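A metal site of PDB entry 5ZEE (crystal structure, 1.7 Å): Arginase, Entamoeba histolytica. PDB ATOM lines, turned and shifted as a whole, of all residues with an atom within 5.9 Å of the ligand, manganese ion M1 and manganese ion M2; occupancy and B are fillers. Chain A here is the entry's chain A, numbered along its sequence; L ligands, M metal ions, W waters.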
ATOM      1  N   HIS A 114      19.859  13.802  10.876  1.00  0.00           N
ATOM      2  CA  HIS A 114      21.106  14.282  10.257  1.00  0.00           C
ATOM      3  C   HIS A 114      21.219  15.785  10.128  1.00  0.00           C
ATOM      4  O   HIS A 114      22.300  16.283   9.770  1.00  0.00           O
ATOM      5  CB  HIS A 114      21.401  13.599   8.909  1.00  0.00           C
ATOM      6  CG  HIS A 114      22.847  13.295   8.704  1.00  0.00           C
ATOM      7  ND1 HIS A 114      23.282  12.393   7.762  1.00  0.00           N
ATOM      8  CD2 HIS A 114      23.945  13.701   9.385  1.00  0.00           C
ATOM      9  CE1 HIS A 114      24.603  12.312   7.836  1.00  0.00           C
ATOM     10  NE2 HIS A 114      25.028  13.071   8.834  1.00  0.00           N
ATOM     11  N   TRP A 138      31.097  11.222   4.624  1.00  0.00           N
ATOM     12  CA  TRP A 138      29.641  11.267   4.847  1.00  0.00           C
ATOM     13  C   TRP A 138      29.103   9.958   4.342  1.00  0.00           C
ATOM     14  O   TRP A 138      28.976   9.753   3.144  1.00  0.00           O
ATOM     15  CB  TRP A 138      29.067  12.463   4.109  1.00  0.00           C
ATOM     16  CG  TRP A 138      27.706  12.850   4.429  1.00  0.00           C
ATOM     17  CD1 TRP A 138      26.556  12.416   3.841  1.00  0.00           C
ATOM     18  CD2 TRP A 138      27.311  13.834   5.377  1.00  0.00           C
ATOM     19  NE1 TRP A 138      25.457  13.064   4.391  1.00  0.00           N
ATOM     20  CE2 TRP A 138      25.901  13.950   5.327  1.00  0.00           C
ATOM     21  CE3 TRP A 138      28.004  14.621   6.287  1.00  0.00           C
ATOM     22  CZ2 TRP A 138      25.170  14.849   6.173  1.00  0.00           C
ATOM     23  CZ3 TRP A 138      27.284  15.495   7.113  1.00  0.00           C
ATOM     24  CH2 TRP A 138      25.893  15.595   7.047  1.00  0.00           C
ATOM     25  N   PHE A 139      28.828   9.041   5.256  1.00  0.00           N
ATOM     26  CA  PHE A 139      28.300   7.726   4.936  1.00  0.00           C
ATOM     27  C   PHE A 139      26.785   7.802   5.057  1.00  0.00           C
ATOM     28  O   PHE A 139      26.241   8.077   6.129  1.00  0.00           O
ATOM     29  CB  PHE A 139      28.859   6.728   5.963  1.00  0.00           C
ATOM     30  CG  PHE A 139      28.415   5.312   5.770  1.00  0.00           C
ATOM     31  CD1 PHE A 139      27.172   4.847   6.232  1.00  0.00           C
ATOM     32  CD2 PHE A 139      29.279   4.395   5.159  1.00  0.00           C
ATOM     33  CE1 PHE A 139      26.770   3.511   6.086  1.00  0.00           C
ATOM     34  CE2 PHE A 139      28.893   3.078   4.995  1.00  0.00           C
ATOM     35  CZ  PHE A 139      27.657   2.620   5.478  1.00  0.00           C
ATOM     36  N   ASP A 140      26.092   7.535   3.954  1.00  0.00           N
ATOM     37  CA  ASP A 140      24.676   7.900   3.876  1.00  0.00           C
ATOM     38  C   ASP A 140      24.075   7.378   2.598  1.00  0.00           C
ATOM     39  O   ASP A 140      24.784   7.202   1.593  1.00  0.00           O
ATOM     40  CB  ASP A 140      24.610   9.432   3.855  1.00  0.00           C
ATOM     41  CG  ASP A 140      23.300   9.986   4.407  1.00  0.00           C
ATOM     42  OD1 ASP A 140      22.217   9.480   4.083  1.00  0.00           O
ATOM     43  OD2 ASP A 140      23.422  10.988   5.133  1.00  0.00           O
ATOM     44  N   ALA A 141      22.790   7.051   2.615  1.00  0.00           N
ATOM     45  CA  ALA A 141      22.022   6.897   1.347  1.00  0.00           C
ATOM     46  C   ALA A 141      21.805   8.232   0.574  1.00  0.00           C
ATOM     47  O   ALA A 141      21.595   8.222  -0.656  1.00  0.00           O
ATOM     48  CB  ALA A 141      20.712   6.229   1.611  1.00  0.00           C
ATOM     49  N   HIS A 142      21.888   9.364   1.291  1.00  0.00           N
ATOM     50  CA  HIS A 142      21.554  10.673   0.754  1.00  0.00           C
ATOM     51  C   HIS A 142      22.747  11.641   0.832  1.00  0.00           C
ATOM     52  O   HIS A 142      23.463  11.647   1.811  1.00  0.00           O
ATOM     53  CB  HIS A 142      20.411  11.287   1.581  1.00  0.00           C
ATOM     54  CG  HIS A 142      19.259  10.381   1.731  1.00  0.00           C
ATOM     55  ND1 HIS A 142      19.103   9.572   2.835  1.00  0.00           N
ATOM     56  CD2 HIS A 142      18.213  10.124   0.913  1.00  0.00           C
ATOM     57  CE1 HIS A 142      18.016   8.820   2.656  1.00  0.00           C
ATOM     58  NE2 HIS A 142      17.449   9.156   1.506  1.00  0.00           N
ATOM     59  N   ASP A 144      22.419  14.892   1.221  1.00  0.00           N
ATOM     60  CA  ASP A 144      22.041  15.921   2.202  1.00  0.00           C
ATOM     61  C   ASP A 144      22.573  17.293   1.784  1.00  0.00           C
ATOM     62  O   ASP A 144      23.028  18.096   2.611  1.00  0.00           O
ATOM     63  CB  ASP A 144      22.538  15.525   3.603  1.00  0.00           C
ATOM     64  CG  ASP A 144      21.790  14.321   4.186  1.00  0.00           C
ATOM     65  OD1 ASP A 144      20.727  13.993   3.640  1.00  0.00           O
ATOM     66  OD2 ASP A 144      22.283  13.655   5.161  1.00  0.00           O
ATOM     67  N   ASN A 146      20.532  19.483  -0.303  1.00  0.00           N
ATOM     68  CA  ASN A 146      19.419  20.241  -0.824  1.00  0.00           C
ATOM     69  C   ASN A 146      19.385  21.594  -0.111  1.00  0.00           C
ATOM     70  O   ASN A 146      20.027  21.782   0.913  1.00  0.00           O
ATOM     71  CB  ASN A 146      18.112  19.505  -0.527  1.00  0.00           C
ATOM     72  CG  ASN A 146      17.876  18.318  -1.452  1.00  0.00           C
ATOM     73  OD1 ASN A 146      18.204  18.372  -2.627  1.00  0.00           O
ATOM     74  ND2 ASN A 146      17.291  17.290  -0.935  1.00  0.00           N
ATOM     75  N   SER A 151      14.352  21.715  -2.076  1.00  0.00           N
ATOM     76  CA  SER A 151      14.064  20.547  -1.227  1.00  0.00           C
ATOM     77  C   SER A 151      12.713  19.972  -1.568  1.00  0.00           C
ATOM     78  O   SER A 151      11.766  20.717  -1.652  1.00  0.00           O
ATOM     79  CB  SER A 151      14.053  20.891   0.259  1.00  0.00           C
ATOM     80  OG  SER A 151      13.567  19.773   0.984  1.00  0.00           O
ATOM     81  N   PRO A 152      12.600  18.646  -1.724  1.00  0.00           N
ATOM     82  CA  PRO A 152      11.244  18.104  -1.955  1.00  0.00           C
ATOM     83  C   PRO A 152      10.371  18.033  -0.723  1.00  0.00           C
ATOM     84  O   PRO A 152       9.191  17.808  -0.845  1.00  0.00           O
ATOM     85  CB  PRO A 152      11.526  16.677  -2.478  1.00  0.00           C
ATOM     86  CG  PRO A 152      12.810  16.304  -1.810  1.00  0.00           C
ATOM     87  CD  PRO A 152      13.632  17.585  -1.730  1.00  0.00           C
ATOM     88  N   SER A 153      10.931  18.187   0.477  1.00  0.00           N
ATOM     89  CA  SER A 153      10.207  17.975   1.713  1.00  0.00           C
ATOM     90  C   SER A 153      10.193  19.173   2.676  1.00  0.00           C
ATOM     91  O   SER A 153       9.349  19.225   3.563  1.00  0.00           O
ATOM     92  CB  SER A 153      10.918  16.821   2.429  1.00  0.00           C
ATOM     93  OG  SER A 153      12.278  17.171   2.778  1.00  0.00           O
ATOM     94  N   GLY A 154      11.134  20.112   2.568  1.00  0.00           N
ATOM     95  CA  GLY A 154      11.347  21.122   3.620  1.00  0.00           C
ATOM     96  C   GLY A 154      12.045  20.639   4.887  1.00  0.00           C
ATOM     97  O   GLY A 154      12.245  21.401   5.833  1.00  0.00           O
ATOM     98  N   ASN A 155      12.475  19.370   4.891  1.00  0.00           N
ATOM     99  CA  ASN A 155      13.101  18.733   6.055  1.00  0.00           C
ATOM    100  C   ASN A 155      14.606  19.075   6.051  1.00  0.00           C
ATOM    101  O   ASN A 155      15.322  18.747   5.128  1.00  0.00           O
ATOM    102  CB  ASN A 155      12.900  17.237   6.031  1.00  0.00           C
ATOM    103  CG  ASN A 155      11.474  16.821   6.260  1.00  0.00           C
ATOM    104  OD1 ASN A 155      10.659  17.565   6.821  1.00  0.00           O
ATOM    105  ND2 ASN A 155      11.165  15.588   5.848  1.00  0.00           N
ATOM    106  N   HIS A 157      17.046  17.943   7.626  1.00  0.00           N
ATOM    107  CA  HIS A 157      18.010  16.850   7.645  1.00  0.00           C
ATOM    108  C   HIS A 157      18.536  16.501   6.271  1.00  0.00           C
ATOM    109  O   HIS A 157      19.565  15.806   6.163  1.00  0.00           O
ATOM    110  CB  HIS A 157      17.471  15.607   8.409  1.00  0.00           C
ATOM    111  CG  HIS A 157      16.483  14.773   7.669  1.00  0.00           C
ATOM    112  ND1 HIS A 157      16.227  13.458   8.015  1.00  0.00           N
ATOM    113  CD2 HIS A 157      15.696  15.049   6.607  1.00  0.00           C
ATOM    114  CE1 HIS A 157      15.327  12.966   7.176  1.00  0.00           C
ATOM    115  NE2 HIS A 157      14.986  13.900   6.310  1.00  0.00           N
ATOM    116  N   GLY A 158      17.925  17.057   5.242  1.00  0.00           N
ATOM    117  CA  GLY A 158      18.396  16.853   3.899  1.00  0.00           C
ATOM    118  C   GLY A 158      19.218  18.017   3.390  1.00  0.00           C
ATOM    119  O   GLY A 158      19.570  18.051   2.264  1.00  0.00           O
ATOM    120  N   MET A 159      19.562  18.941   4.277  1.00  0.00           N
ATOM    121  CA  MET A 159      20.313  20.135   3.913  1.00  0.00           C
ATOM    122  C   MET A 159      21.651  20.444   4.590  1.00  0.00           C
ATOM    123  O   MET A 159      22.307  21.349   4.188  1.00  0.00           O
ATOM    124  CB  MET A 159      19.426  21.355   4.162  1.00  0.00           C
ATOM    125  CG  MET A 159      18.048  21.321   3.554  1.00  0.00           C
ATOM    126  SD  MET A 159      17.115  22.796   4.017  1.00  0.00           S
ATOM    127  CE  MET A 159      15.493  22.226   3.638  1.00  0.00           C
ATOM    128  N   SER A 192      20.200   7.768  -3.208  1.00  0.00           N
ATOM    129  CA  SER A 192      18.965   8.476  -3.404  1.00  0.00           C
ATOM    130  C   SER A 192      19.373   9.928  -3.567  1.00  0.00           C
ATOM    131  O   SER A 192      19.573  10.617  -2.625  1.00  0.00           O
ATOM    132  CB  SER A 192      18.013   8.275  -2.232  1.00  0.00           C
ATOM    133  OG  SER A 192      16.886   9.081  -2.336  1.00  0.00           O
ATOM    134  N   ASP A 194      18.799  13.774  -5.360  1.00  0.00           N
ATOM    135  CA  ASP A 194      17.872  14.694  -5.980  1.00  0.00           C
ATOM    136  C   ASP A 194      18.524  15.511  -7.080  1.00  0.00           C
ATOM    137  O   ASP A 194      19.706  15.517  -7.205  1.00  0.00           O
ATOM    138  CB  ASP A 194      17.261  15.628  -4.948  1.00  0.00           C
ATOM    139  CG  ASP A 194      16.350  14.929  -3.981  1.00  0.00           C
ATOM    140  OD1 ASP A 194      15.727  13.929  -4.338  1.00  0.00           O
ATOM    141  OD2 ASP A 194      16.231  15.381  -2.862  1.00  0.00           O
ATOM    142  N   GLU A 197      21.289  17.924  -5.981  1.00  0.00           N
ATOM    143  CA  GLU A 197      22.416  17.224  -5.426  1.00  0.00           C
ATOM    144  C   GLU A 197      23.282  16.627  -6.533  1.00  0.00           C
ATOM    145  O   GLU A 197      24.486  16.711  -6.484  1.00  0.00           O
ATOM    146  CB  GLU A 197      21.964  16.159  -4.451  1.00  0.00           C
ATOM    147  CG  GLU A 197      21.147  16.747  -3.277  1.00  0.00           C
ATOM    148  CD  GLU A 197      20.600  15.658  -2.376  1.00  0.00           C
ATOM    149  OE1 GLU A 197      19.904  14.708  -2.905  1.00  0.00           O
ATOM    150  OE2 GLU A 197      20.861  15.754  -1.150  1.00  0.00           O
ATOM    151  N   ASP A 241      25.342   8.130   8.822  1.00  0.00           N
ATOM    152  CA  ASP A 241      23.926   7.924   8.766  1.00  0.00           C
ATOM    153  C   ASP A 241      23.669   6.452   8.558  1.00  0.00           C
ATOM    154  O   ASP A 241      24.086   5.840   7.567  1.00  0.00           O
ATOM    155  CB  ASP A 241      23.365   8.758   7.598  1.00  0.00           C
ATOM    156  CG  ASP A 241      21.845   8.852   7.585  1.00  0.00           C
ATOM    157  OD1 ASP A 241      21.162   7.880   8.020  1.00  0.00           O
ATOM    158  OD2 ASP A 241      21.340   9.893   7.064  1.00  0.00           O
ATOM    159  N   ASP A 243      21.204   4.893   7.600  1.00  0.00           N
ATOM    160  CA  ASP A 243      20.465   4.502   6.378  1.00  0.00           C
ATOM    161  C   ASP A 243      21.370   4.297   5.140  1.00  0.00           C
ATOM    162  O   ASP A 243      20.914   3.862   4.100  1.00  0.00           O
ATOM    163  CB  ASP A 243      19.282   5.406   6.094  1.00  0.00           C
ATOM    164  CG  ASP A 243      19.629   6.786   5.572  1.00  0.00           C
ATOM    165  OD1 ASP A 243      20.740   7.060   5.025  1.00  0.00           O
ATOM    166  OD2 ASP A 243      18.706   7.647   5.738  1.00  0.00           O
ATOM    167  N   GLY A 244      22.641   4.607   5.289  1.00  0.00           N
ATOM    168  CA  GLY A 244      23.655   4.113   4.318  1.00  0.00           C
ATOM    169  C   GLY A 244      23.618   2.608   4.170  1.00  0.00           C
ATOM    170  O   GLY A 244      23.871   2.046   3.079  1.00  0.00           O
ATOM    171  N   THR A 255      14.099   7.173   6.639  1.00  0.00           N
ATOM    172  CA  THR A 255      14.149   7.199   5.190  1.00  0.00           C
ATOM    173  C   THR A 255      15.032   6.054   4.661  1.00  0.00           C
ATOM    174  O   THR A 255      16.110   6.312   4.105  1.00  0.00           O
ATOM    175  CB  THR A 255      14.699   8.546   4.690  1.00  0.00           C
ATOM    176  OG1 THR A 255      15.979   8.805   5.291  1.00  0.00           O
ATOM    177  CG2 THR A 255      13.734   9.721   5.073  1.00  0.00           C
ATOM    178  N   VAL A 285      23.917   8.822  13.330  1.00  0.00           N
ATOM    179  CA  VAL A 285      22.622   9.473  13.211  1.00  0.00           C
ATOM    180  C   VAL A 285      21.545   8.617  12.571  1.00  0.00           C
ATOM    181  O   VAL A 285      21.811   7.645  11.879  1.00  0.00           O
ATOM    182  CB  VAL A 285      22.731  10.792  12.425  1.00  0.00           C
ATOM    183  CG1 VAL A 285      23.696  11.779  13.097  1.00  0.00           C
ATOM    184  CG2 VAL A 285      23.080  10.576  10.964  1.00  0.00           C
ATOM    185  N   GLU A 286      20.304   9.029  12.845  1.00  0.00           N
ATOM    186  CA  GLU A 286      19.090   8.563  12.212  1.00  0.00           C
ATOM    187  C   GLU A 286      18.537   7.242  12.738  1.00  0.00           C
ATOM    188  O   GLU A 286      17.662   6.672  12.119  1.00  0.00           O
ATOM    189  CB  GLU A 286      19.172   8.598  10.663  1.00  0.00           C
ATOM    190  CG  GLU A 286      19.361   9.979  10.042  1.00  0.00           C
ATOM    191  CD  GLU A 286      18.062  10.869  10.018  1.00  0.00           C
ATOM    192  OE1 GLU A 286      16.958  10.426  10.444  1.00  0.00           O
ATOM    193  OE2 GLU A 286      18.127  12.024   9.487  1.00  0.00           O
HETATM  194  N1  LIG L   1      16.435  14.055  -0.185  1.00  0.00           N
HETATM  195  C1  LIG L   1      15.358  13.872   0.854  1.00  0.00           C
HETATM  196  C2  LIG L   1      14.822  15.225   1.362  1.00  0.00           C
HETATM  197  O1  LIG L   1      13.651  15.171   1.826  1.00  0.00           O
HETATM  198  C3  LIG L   1      15.870  13.047   2.025  1.00  0.00           C
HETATM  199  C4  LIG L   1      17.226  13.610   2.514  1.00  0.00           C
HETATM  200  C5  LIG L   1      17.631  13.336   3.943  1.00  0.00           C
HETATM  201  N2  LIG L   1      17.614  12.118   4.410  1.00  0.00           N
HETATM  202  C6  LIG L   1      18.079  11.885   5.780  1.00  0.00           C
HETATM  203  N3  LIG L   1      19.525  12.246   5.814  1.00  0.00           N
HETATM  204  N4  LIG L   1      17.737  10.544   6.194  1.00  0.00           N
HETATM  205  O2  LIG L   1      20.520  11.362   5.351  1.00  0.00           O
HETATM  206  O3  LIG L   1      15.583  16.260   1.257  1.00  0.00           O
HETATM  207 MN    MN M   1      20.104   9.520   5.107  1.00  0.00          MN
HETATM  208 MN    MN M   2      22.109  11.863   6.277  1.00  0.00          MN
HETATM  209  O   HOH W   1      18.618  12.761  -1.435  1.00  0.00           O
HETATM  210  O   HOH W   2      15.374  18.651   2.391  1.00  0.00           O
HETATM  211  O   HOH W   3      16.733   7.714   7.686  1.00  0.00           O
HETATM  212  O   HOH W   4      12.961  13.709   4.569  1.00  0.00           O
HETATM  213  O   HOH W   5      15.292   9.945   8.478  1.00  0.00           O
HETATM  214  O   HOH W   6      19.022  15.220   0.602  1.00  0.00           O
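Water W2 lies within hydrogen-bond range of OG of Ser 151 (2.6 Å), O3 of the ligand (2.7 Å), O of Asn 155 (2.7 Å) and OG of Ser 153 (3.5 Å).
Water W1 lies within hydrogen-bond range of the backbone carbonyl oxygen (O) of Ser 192 (2.6 Å), the side-chain carboxylate (OE1) of Glu 197 (2.8 Å) and a nitrogen (N1) of the ligand (2.8 Å).
Water W6 lies within hydrogen-bond range of OE2 of Glu 197, N1 of the ligand, ND2 of Asn 146, O of Gly 158 and N of Asp 144.
Water W4 lies within hydrogen-bond range of a ring nitrogen (NE2) of His 157, the side-chain amide nitrogen of Asn 155 and an oxygen (O1) of the ligand.
Water W3 bridges OG1 of Thr 255 (2.7 Å) and N4 of the ligand (3.4 Å).
Water W5 lies within hydrogen-bond range of OE1 of Glu 286 (2.6 Å), N4 of the ligand (3.4 Å) and OG1 of Thr 255 (3.5 Å).
Manganese ion M2 is bound by O2 of the ligand, OD2 of Asp 140, ND1 of His 114, OD2 of Asp 144 and OD2 of Asp 241.
An oxygen (O2) of the ligand is bound to manganese ion M1, 1.9 Å away.
The side-chain carboxylate (OD2) of Asp 241 binds manganese ion M1 (2.3 Å).
OD1 of Asp 140 binds manganese ion M1, 2.3 Å away.
OD2 of Asp 243 binds manganese ion M1, at 2.4 Å.
Manganese ion M1 is bound by ND1 of His 142 (2.5 Å).
Manganese ion M1 is bound by the side-chain carboxylate (OD1) of Asp 243 (2.5 Å).
Slightly farther from manganese ion M1 lies a nitrogen (N4) of the ligand (2.8 Å).
Within 4 Å of manganese ion M1: Asp 140, His 142, Asp 241 and Asp 243.
The backbone NH (N) of Asp 144 is in hydrogen-bond range of the side-chain carboxylate (OE2) of Glu 197.
The side-chain carboxylate (OE2) of Glu 286 sits at hydrogen-bond distance from the backbone NH (N) of His 114, at 2.8 Å.
The side-chain carboxylate (OD2) of Asp 140 sits close to the indole nitrogen (NE1) of Trp 138 (3.0 Å).
N of Asp 194 sits at hydrogen-bond distance from OE1 of Glu 197.
The side-chain hydroxyl (OG) of Ser 151 lies within hydrogen-bond range of the backbone NH (N) of Ser 153 (3.1 Å).
O of Gly 158 sits at hydrogen-bond distance from N of Asn 146 (3.1 Å).
OD2 of Asp 194 sits at hydrogen-bond distance from ND2 of Asn 146 (2.9 Å).
N of Asn 155 is in hydrogen-bond range of OG of Ser 153, 3.1 Å away.
The side-chain hydroxyl (OG) of Ser 153 sits at hydrogen-bond distance from an oxygen (O1) of the ligand (2.6 Å).
OG1 of Thr 255 sits at hydrogen-bond distance from N4 of the ligand, at 2.6 Å.
The side-chain carboxylate of Asp 194 lies within salt-bridge range of a nitrogen (N1) of the ligand, 3.0 Å away.
The side-chain amide nitrogen (ND2) of Asn 146 is in hydrogen-bond range of an oxygen (O3) of the ligand (3.0 Å).
OE2 of Glu 286 is in salt-bridge range of N4 of the ligand, at 3.6 Å.
CD of Pro 152 touches O3 of the ligand, at 3.8 Å.
His 157 touches the ligand.
Gly 158 touches the ligand (CA to C5, 3.6 Å).
Of the 25 residues printed, 14 come within 4 Å of the ligand.
The nearest printed residue that does not touch the ligand is Ser 151 (4.1 Å).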
